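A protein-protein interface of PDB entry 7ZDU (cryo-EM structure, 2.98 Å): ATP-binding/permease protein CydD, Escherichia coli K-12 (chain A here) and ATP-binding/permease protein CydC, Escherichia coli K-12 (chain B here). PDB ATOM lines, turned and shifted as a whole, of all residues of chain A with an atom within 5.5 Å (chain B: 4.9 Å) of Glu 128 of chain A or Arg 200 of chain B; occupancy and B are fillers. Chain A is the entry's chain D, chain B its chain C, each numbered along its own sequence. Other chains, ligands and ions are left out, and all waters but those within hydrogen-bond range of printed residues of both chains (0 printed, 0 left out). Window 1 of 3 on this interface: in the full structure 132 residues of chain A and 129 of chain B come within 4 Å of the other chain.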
ATOM      1  N   ALA A 123      17.674 -22.622  12.659  1.00  0.00           N
ATOM      2  CA  ALA A 123      16.656 -22.305  13.654  1.00  0.00           C
ATOM      3  C   ALA A 123      15.649 -21.297  13.122  1.00  0.00           C
ATOM      4  O   ALA A 123      14.442 -21.444  13.339  1.00  0.00           O
ATOM      5  CB  ALA A 123      17.315 -21.780  14.926  1.00  0.00           C
ATOM      6  N   THR A 124      16.120 -20.263  12.429  1.00  0.00           N
ATOM      7  CA  THR A 124      15.202 -19.287  11.857  1.00  0.00           C
ATOM      8  C   THR A 124      14.459 -19.840  10.651  1.00  0.00           C
ATOM      9  O   THR A 124      13.377 -19.347  10.324  1.00  0.00           O
ATOM     10  CB  THR A 124      15.957 -18.018  11.472  1.00  0.00           C
ATOM     11  OG1 THR A 124      15.066 -17.108  10.819  1.00  0.00           O
ATOM     12  CG2 THR A 124      17.090 -18.351  10.548  1.00  0.00           C
ATOM     13  N   LEU A 125      15.020 -20.845   9.984  1.00  0.00           N
ATOM     14  CA  LEU A 125      14.293 -21.534   8.927  1.00  0.00           C
ATOM     15  C   LEU A 125      13.138 -22.347   9.496  1.00  0.00           C
ATOM     16  O   LEU A 125      12.060 -22.409   8.896  1.00  0.00           O
ATOM     17  CB  LEU A 125      15.259 -22.417   8.138  1.00  0.00           C
ATOM     18  CG  LEU A 125      14.792 -23.203   6.918  1.00  0.00           C
ATOM     19  CD1 LEU A 125      15.921 -23.329   5.925  1.00  0.00           C
ATOM     20  CD2 LEU A 125      14.368 -24.582   7.356  1.00  0.00           C
ATOM     21  N   VAL A 126      13.345 -22.975  10.654  1.00  0.00           N
ATOM     22  CA  VAL A 126      12.309 -23.821  11.234  1.00  0.00           C
ATOM     23  C   VAL A 126      11.333 -22.992  12.053  1.00  0.00           C
ATOM     24  O   VAL A 126      10.122 -23.229  12.022  1.00  0.00           O
ATOM     25  CB  VAL A 126      12.948 -24.941  12.075  1.00  0.00           C
ATOM     26  CG1 VAL A 126      11.883 -25.842  12.662  1.00  0.00           C
ATOM     27  CG2 VAL A 126      13.911 -25.750  11.232  1.00  0.00           C
ATOM     28  N   LEU A 127      11.837 -22.015  12.805  1.00  0.00           N
ATOM     29  CA  LEU A 127      10.953 -21.223  13.652  1.00  0.00           C
ATOM     30  C   LEU A 127      10.304 -20.079  12.885  1.00  0.00           C
ATOM     31  O   LEU A 127       9.082 -20.042  12.724  1.00  0.00           O
ATOM     32  CB  LEU A 127      11.721 -20.677  14.856  1.00  0.00           C
ATOM     33  CG  LEU A 127      12.225 -21.701  15.863  1.00  0.00           C
ATOM     34  CD1 LEU A 127      12.387 -21.058  17.217  1.00  0.00           C
ATOM     35  CD2 LEU A 127      11.249 -22.835  15.931  1.00  0.00           C
ATOM     36  N   GLU A 128      11.112 -19.140  12.394  1.00  0.00           N
ATOM     37  CA  GLU A 128      10.558 -17.897  11.869  1.00  0.00           C
ATOM     38  C   GLU A 128       9.920 -18.094  10.501  1.00  0.00           C
ATOM     39  O   GLU A 128       8.840 -17.557  10.235  1.00  0.00           O
ATOM     40  CB  GLU A 128      11.645 -16.830  11.804  1.00  0.00           C
ATOM     41  CG  GLU A 128      11.723 -15.967  13.046  1.00  0.00           C
ATOM     42  CD  GLU A 128      12.356 -16.695  14.215  1.00  0.00           C
ATOM     43  OE1 GLU A 128      13.264 -17.517  13.982  1.00  0.00           O
ATOM     44  OE2 GLU A 128      11.942 -16.446  15.367  1.00  0.00           O
ATOM     45  N   GLN A 129      10.568 -18.856   9.621  1.00  0.00           N
ATOM     46  CA  GLN A 129      10.079 -18.960   8.252  1.00  0.00           C
ATOM     47  C   GLN A 129       8.820 -19.812   8.156  1.00  0.00           C
ATOM     48  O   GLN A 129       7.970 -19.556   7.297  1.00  0.00           O
ATOM     49  CB  GLN A 129      11.176 -19.512   7.344  1.00  0.00           C
ATOM     50  CG  GLN A 129      12.359 -18.576   7.194  1.00  0.00           C
ATOM     51  CD  GLN A 129      13.252 -18.942   6.033  1.00  0.00           C
ATOM     52  OE1 GLN A 129      12.850 -19.679   5.137  1.00  0.00           O
ATOM     53  NE2 GLN A 129      14.474 -18.431   6.043  1.00  0.00           N
ATOM     54  N   ILE A 130       8.673 -20.816   9.017  1.00  0.00           N
ATOM     55  CA  ILE A 130       7.462 -21.627   8.985  1.00  0.00           C
ATOM     56  C   ILE A 130       6.327 -20.933   9.729  1.00  0.00           C
ATOM     57  O   ILE A 130       5.167 -20.998   9.314  1.00  0.00           O
ATOM     58  CB  ILE A 130       7.745 -23.029   9.548  1.00  0.00           C
ATOM     59  CG1 ILE A 130       8.670 -23.793   8.608  1.00  0.00           C
ATOM     60  CG2 ILE A 130       6.464 -23.804   9.720  1.00  0.00           C
ATOM     61  CD1 ILE A 130       9.057 -25.153   9.107  1.00  0.00           C
ATOM     62  N   ASP A 131       6.639 -20.245  10.828  1.00  0.00           N
ATOM     63  CA  ASP A 131       5.611 -19.523  11.563  1.00  0.00           C
ATOM     64  C   ASP A 131       5.088 -18.318  10.797  1.00  0.00           C
ATOM     65  O   ASP A 131       4.021 -17.802  11.138  1.00  0.00           O
ATOM     66  CB  ASP A 131       6.146 -19.068  12.919  1.00  0.00           C
ATOM     67  CG  ASP A 131       5.780 -20.018  14.038  1.00  0.00           C
ATOM     68  OD1 ASP A 131       5.134 -21.049  13.762  1.00  0.00           O
ATOM     69  OD2 ASP A 131       6.140 -19.733  15.199  1.00  0.00           O
ATOM     70  N   ASP A 132       5.811 -17.855   9.781  1.00  0.00           N
ATOM     71  CA  ASP A 132       5.402 -16.689   9.011  1.00  0.00           C
ATOM     72  C   ASP A 132       4.560 -17.044   7.796  1.00  0.00           C
ATOM     73  O   ASP A 132       4.201 -16.149   7.026  1.00  0.00           O
ATOM     74  CB  ASP A 132       6.627 -15.886   8.578  1.00  0.00           C
ATOM     75  CG  ASP A 132       7.176 -15.026   9.696  1.00  0.00           C
ATOM     76  OD1 ASP A 132       8.150 -14.286   9.459  1.00  0.00           O
ATOM     77  OD2 ASP A 132       6.637 -15.093  10.819  1.00  0.00           O
ATOM     78  N   MET A 133       4.240 -18.318   7.604  1.00  0.00           N
ATOM     79  CA  MET A 133       3.247 -18.722   6.623  1.00  0.00           C
ATOM     80  C   MET A 133       1.856 -18.848   7.219  1.00  0.00           C
ATOM     81  O   MET A 133       0.933 -19.263   6.513  1.00  0.00           O
ATOM     82  CB  MET A 133       3.640 -20.049   5.975  1.00  0.00           C
ATOM     83  CG  MET A 133       5.096 -20.160   5.613  1.00  0.00           C
ATOM     84  SD  MET A 133       5.490 -21.771   4.929  1.00  0.00           S
ATOM     85  CE  MET A 133       7.151 -21.473   4.358  1.00  0.00           C
ATOM     86  N   PHE A 195      14.283 -12.607   5.078  1.00  0.00           N
ATOM     87  CA  PHE A 195      14.603 -13.829   5.799  1.00  0.00           C
ATOM     88  C   PHE A 195      16.027 -14.291   5.551  1.00  0.00           C
ATOM     89  O   PHE A 195      16.545 -15.104   6.322  1.00  0.00           O
ATOM     90  CB  PHE A 195      13.627 -14.938   5.414  1.00  0.00           C
ATOM     91  CG  PHE A 195      12.228 -14.690   5.872  1.00  0.00           C
ATOM     92  CD1 PHE A 195      11.905 -14.772   7.211  1.00  0.00           C
ATOM     93  CD2 PHE A 195      11.237 -14.375   4.967  1.00  0.00           C
ATOM     94  CE1 PHE A 195      10.620 -14.541   7.635  1.00  0.00           C
ATOM     95  CE2 PHE A 195       9.951 -14.144   5.386  1.00  0.00           C
ATOM     96  CZ  PHE A 195       9.642 -14.228   6.720  1.00  0.00           C
ATOM     97  N   LEU A 198      17.886 -12.120   8.148  1.00  0.00           N
ATOM     98  CA  LEU A 198      17.621 -12.652   9.480  1.00  0.00           C
ATOM     99  C   LEU A 198      18.387 -13.944   9.716  1.00  0.00           C
ATOM    100  O   LEU A 198      18.970 -14.139  10.787  1.00  0.00           O
ATOM    101  CB  LEU A 198      16.124 -12.875   9.665  1.00  0.00           C
ATOM    102  CG  LEU A 198      15.676 -13.491  10.988  1.00  0.00           C
ATOM    103  CD1 LEU A 198      16.207 -12.695  12.166  1.00  0.00           C
ATOM    104  CD2 LEU A 198      14.164 -13.582  11.043  1.00  0.00           C
ATOM    105  N   ALA A 320       9.360 -16.733   2.624  1.00  0.00           N
ATOM    106  CA  ALA A 320       9.725 -17.712   3.637  1.00  0.00           C
ATOM    107  C   ALA A 320       9.818 -19.126   3.089  1.00  0.00           C
ATOM    108  O   ALA A 320      10.461 -19.974   3.712  1.00  0.00           O
ATOM    109  CB  ALA A 320       8.719 -17.674   4.787  1.00  0.00           C
ATOM    110  N   GLY B 117      21.361 -22.005  22.659  1.00  0.00           N
ATOM    111  CA  GLY B 117      20.183 -21.840  21.826  1.00  0.00           C
ATOM    112  C   GLY B 117      19.151 -20.908  22.428  1.00  0.00           C
ATOM    113  O   GLY B 117      18.415 -20.240  21.701  1.00  0.00           O
ATOM    114  N   LEU B 120      20.499 -17.338  21.948  1.00  0.00           N
ATOM    115  CA  LEU B 120      20.192 -16.891  20.596  1.00  0.00           C
ATOM    116  C   LEU B 120      18.754 -16.412  20.490  1.00  0.00           C
ATOM    117  O   LEU B 120      18.454 -15.510  19.704  1.00  0.00           O
ATOM    118  CB  LEU B 120      20.470 -18.020  19.602  1.00  0.00           C
ATOM    119  CG  LEU B 120      19.767 -18.035  18.245  1.00  0.00           C
ATOM    120  CD1 LEU B 120      20.265 -16.908  17.363  1.00  0.00           C
ATOM    121  CD2 LEU B 120      19.966 -19.377  17.568  1.00  0.00           C
ATOM    122  N   ASN B 121      17.854 -17.000  21.276  1.00  0.00           N
ATOM    123  CA  ASN B 121      16.476 -16.530  21.308  1.00  0.00           C
ATOM    124  C   ASN B 121      16.381 -15.132  21.904  1.00  0.00           C
ATOM    125  O   ASN B 121      15.624 -14.292  21.407  1.00  0.00           O
ATOM    126  CB  ASN B 121      15.609 -17.507  22.097  1.00  0.00           C
ATOM    127  CG  ASN B 121      14.137 -17.290  21.864  1.00  0.00           C
ATOM    128  OD1 ASN B 121      13.620 -17.579  20.789  1.00  0.00           O
ATOM    129  ND2 ASN B 121      13.449 -16.775  22.872  1.00  0.00           N
ATOM    130  N   ALA B 125      15.426 -12.981  18.923  1.00  0.00           N
ATOM    131  CA  ALA B 125      13.970 -13.063  18.909  1.00  0.00           C
ATOM    132  C   ALA B 125      13.320 -12.237  20.014  1.00  0.00           C
ATOM    133  O   ALA B 125      12.365 -11.500  19.756  1.00  0.00           O
ATOM    134  CB  ALA B 125      13.526 -14.522  19.017  1.00  0.00           C
ATOM    135  N   ARG B 196       8.968 -20.723  23.020  1.00  0.00           N
ATOM    136  CA  ARG B 196       9.700 -20.384  21.805  1.00  0.00           C
ATOM    137  C   ARG B 196      11.201 -20.482  22.030  1.00  0.00           C
ATOM    138  O   ARG B 196      11.935 -20.966  21.160  1.00  0.00           O
ATOM    139  CB  ARG B 196       9.324 -18.985  21.326  1.00  0.00           C
ATOM    140  CG  ARG B 196       9.987 -18.599  20.017  1.00  0.00           C
ATOM    141  CD  ARG B 196       9.546 -17.230  19.554  1.00  0.00           C
ATOM    142  NE  ARG B 196       9.825 -16.212  20.557  1.00  0.00           N
ATOM    143  CZ  ARG B 196       9.664 -14.908  20.364  1.00  0.00           C
ATOM    144  NH1 ARG B 196       9.220 -14.458  19.200  1.00  0.00           N
ATOM    145  NH2 ARG B 196       9.945 -14.055  21.337  1.00  0.00           N
ATOM    146  N   GLY B 197      11.676 -20.022  23.188  1.00  0.00           N
ATOM    147  CA  GLY B 197      13.085 -20.150  23.504  1.00  0.00           C
ATOM    148  C   GLY B 197      13.487 -21.566  23.855  1.00  0.00           C
ATOM    149  O   GLY B 197      14.643 -21.949  23.664  1.00  0.00           O
ATOM    150  N   GLN B 198      12.526 -22.350  24.348  1.00  0.00           N
ATOM    151  CA  GLN B 198      12.796 -23.767  24.705  1.00  0.00           C
ATOM    152  C   GLN B 198      12.898 -24.590  23.419  1.00  0.00           C
ATOM    153  O   GLN B 198      13.782 -25.456  23.349  1.00  0.00           O
ATOM    154  CB  GLN B 198      11.705 -24.312  25.622  1.00  0.00           C
ATOM    155  CG  GLN B 198      11.909 -25.774  25.983  1.00  0.00           C
ATOM    156  CD  GLN B 198      11.073 -26.189  27.166  1.00  0.00           C
ATOM    157  OE1 GLN B 198      10.944 -25.457  28.143  1.00  0.00           O
ATOM    158  NE2 GLN B 198      10.499 -27.377  27.086  1.00  0.00           N
ATOM    159  N   TYR B 199      12.039 -24.311  22.433  1.00  0.00           N
ATOM    160  CA  TYR B 199      12.095 -25.040  21.171  1.00  0.00           C
ATOM    161  C   TYR B 199      13.370 -24.717  20.405  1.00  0.00           C
ATOM    162  O   TYR B 199      13.985 -25.610  19.814  1.00  0.00           O
ATOM    163  CB  TYR B 199      10.868 -24.726  20.319  1.00  0.00           C
ATOM    164  CG  TYR B 199      10.698 -25.660  19.144  1.00  0.00           C
ATOM    165  CD1 TYR B 199       9.877 -26.767  19.225  1.00  0.00           C
ATOM    166  CD2 TYR B 199      11.376 -25.444  17.958  1.00  0.00           C
ATOM    167  CE1 TYR B 199       9.727 -27.620  18.157  1.00  0.00           C
ATOM    168  CE2 TYR B 199      11.231 -26.291  16.885  1.00  0.00           C
ATOM    169  CZ  TYR B 199      10.406 -27.378  16.990  1.00  0.00           C
ATOM    170  OH  TYR B 199      10.260 -28.230  15.923  1.00  0.00           O
ATOM    171  N   ARG B 200      13.777 -23.448  20.397  1.00  0.00           N
ATOM    172  CA  ARG B 200      14.994 -23.073  19.687  1.00  0.00           C
ATOM    173  C   ARG B 200      16.222 -23.705  20.326  1.00  0.00           C
ATOM    174  O   ARG B 200      17.166 -24.080  19.625  1.00  0.00           O
ATOM    175  CB  ARG B 200      15.139 -21.555  19.641  1.00  0.00           C
ATOM    176  CG  ARG B 200      16.105 -21.080  18.579  1.00  0.00           C
ATOM    177  CD  ARG B 200      16.329 -19.591  18.654  1.00  0.00           C
ATOM    178  NE  ARG B 200      15.081 -18.854  18.805  1.00  0.00           N
ATOM    179  CZ  ARG B 200      14.413 -18.306  17.800  1.00  0.00           C
ATOM    180  NH1 ARG B 200      14.872 -18.415  16.563  1.00  0.00           N
ATOM    181  NH2 ARG B 200      13.285 -17.653  18.029  1.00  0.00           N
ATOM    182  N   GLN B 201      16.231 -23.823  21.653  1.00  0.00           N
ATOM    183  CA  GLN B 201      17.341 -24.496  22.315  1.00  0.00           C
ATOM    184  C   GLN B 201      17.359 -25.981  21.990  1.00  0.00           C
ATOM    185  O   GLN B 201      18.406 -26.535  21.642  1.00  0.00           O
ATOM    186  CB  GLN B 201      17.260 -24.289  23.824  1.00  0.00           C
ATOM    187  CG  GLN B 201      18.613 -24.185  24.484  1.00  0.00           C
ATOM    188  CD  GLN B 201      19.414 -25.466  24.383  1.00  0.00           C
ATOM    189  OE1 GLN B 201      18.918 -26.549  24.690  1.00  0.00           O
ATOM    190  NE2 GLN B 201      20.660 -25.350  23.939  1.00  0.00           N
ATOM    191  N   GLN B 202      16.208 -26.642  22.097  1.00  0.00           N
ATOM    192  CA  GLN B 202      16.141 -28.070  21.829  1.00  0.00           C
ATOM    193  C   GLN B 202      16.354 -28.395  20.360  1.00  0.00           C
ATOM    194  O   GLN B 202      16.709 -29.531  20.039  1.00  0.00           O
ATOM    195  CB  GLN B 202      14.801 -28.623  22.299  1.00  0.00           C
ATOM    196  CG  GLN B 202      14.626 -28.598  23.797  1.00  0.00           C
ATOM    197  CD  GLN B 202      13.315 -29.198  24.233  1.00  0.00           C
ATOM    198  OE1 GLN B 202      12.342 -29.189  23.486  1.00  0.00           O
ATOM    199  NE2 GLN B 202      13.280 -29.726  25.447  1.00  0.00           N
ATOM    200  N   LEU B 203      16.140 -27.431  19.464  1.00  0.00           N
ATOM    201  CA  LEU B 203      16.378 -27.666  18.045  1.00  0.00           C
ATOM    202  C   LEU B 203      17.849 -27.500  17.692  1.00  0.00           C
ATOM    203  O   LEU B 203      18.427 -28.346  17.004  1.00  0.00           O
ATOM    204  CB  LEU B 203      15.521 -26.722  17.205  1.00  0.00           C
ATOM    205  CG  LEU B 203      15.742 -26.809  15.698  1.00  0.00           C
ATOM    206  CD1 LEU B 203      14.975 -27.976  15.120  1.00  0.00           C
ATOM    207  CD2 LEU B 203      15.337 -25.514  15.034  1.00  0.00           C
ATOM    208  N   THR B 204      18.472 -26.412  18.151  1.00  0.00           N
ATOM    209  CA  THR B 204      19.881 -26.193  17.847  1.00  0.00           C
ATOM    210  C   THR B 204      20.766 -27.228  18.524  1.00  0.00           C
ATOM    211  O   THR B 204      21.804 -27.606  17.973  1.00  0.00           O
ATOM    212  CB  THR B 204      20.304 -24.783  18.254  1.00  0.00           C
ATOM    213  OG1 THR B 204      20.106 -24.604  19.660  1.00  0.00           O
ATOM    214  CG2 THR B 204      19.493 -23.747  17.499  1.00  0.00           C
ATOM    215  N   ALA B 205      20.380 -27.693  19.713  1.00  0.00           N
ATOM    216  CA  ALA B 205      21.115 -28.781  20.348  1.00  0.00           C
ATOM    217  C   ALA B 205      20.903 -30.091  19.604  1.00  0.00           C
ATOM    218  O   ALA B 205      21.817 -30.917  19.516  1.00  0.00           O
ATOM    219  CB  ALA B 205      20.692 -28.918  21.808  1.00  0.00           C
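The guanidinium group (NH1) of Arg 200 of chain B lies within salt-bridge range of the side-chain carboxylate (OE1) of Glu 128 of chain A, at 3.2 Å.
NE of Arg 200 of chain B sits at hydrogen-bond distance from OD1 of Asn 121 of chain B, 2.8 Å away. The backbone carbonyl oxygen (O) of Arg 200 of chain B lies within hydrogen-bond range of the side-chain hydroxyl (OG1) of Thr 204 of chain B, 3.0 Å away. The side-chain hydroxyl (OG1) of Thr 204 of chain B sits at hydrogen-bond distance from the backbone carbonyl oxygen (O) of Gln 201 of chain B, 3.2 Å away.
Among the printed residues, merely in contact across the chains: Ala 123 of chain A with Arg 200 of chain B, Ala 123 of chain A with Leu 203 of chain B, Ala 123 of chain A with Thr 204 of chain B, Val 126 of chain A with Leu 203 of chain B, Leu 127 of chain A with Arg 196 of chain B, Leu 127 of chain A with Tyr 199 of chain B and Leu 127 of chain A with Arg 200 of chain B.
Printed residues of chain B within 4 Å of Glu 128 of chain A: Arg 200 (3.2 Å). Of chain A, only Ala 123 (3.9 Å), Leu 127 (3.5 Å) and Glu 128 (3.2 Å) come within 4 Å of Arg 200 of chain B. Of the printed residues of chain A, Arg 196 of chain B touches Leu 127 (3.97 Å). Of the printed residues of chain A, Tyr 199 of chain B touches Leu 127 (3.3 Å). Printed residues of chain B within 4 Å of Leu 127 of chain A: Arg 196, Tyr 199 and Arg 200. Of the printed residues of chain B, Ala 123 of chain A touches Arg 200 (3.9 Å), Leu 203 (3.7 Å) and Thr 204 (3.9 Å). Leu 120 of chain B touches none of the printed residues of chain A. The nearest residue of chain B that does not touch Glu 128 of chain A is Ala 125 of chain B (4.4 Å).
Of the 14 printed residues of chain A, 4 touch a printed residue of chain B. Hydrophobic or aromatic side chains of chain A within 4 Å of the printed part of chain B: Ala 123, Val 126 and Leu 127. Along chain A the printed residues that touch a printed residue of chain B span positions 123 to 128. Of the 14 printed residues of chain B, 5 touch a printed residue of chain A. Hydrophobic or aromatic side chains of chain B within 4 Å of the printed part of chain A: Tyr 199 and Leu 203.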
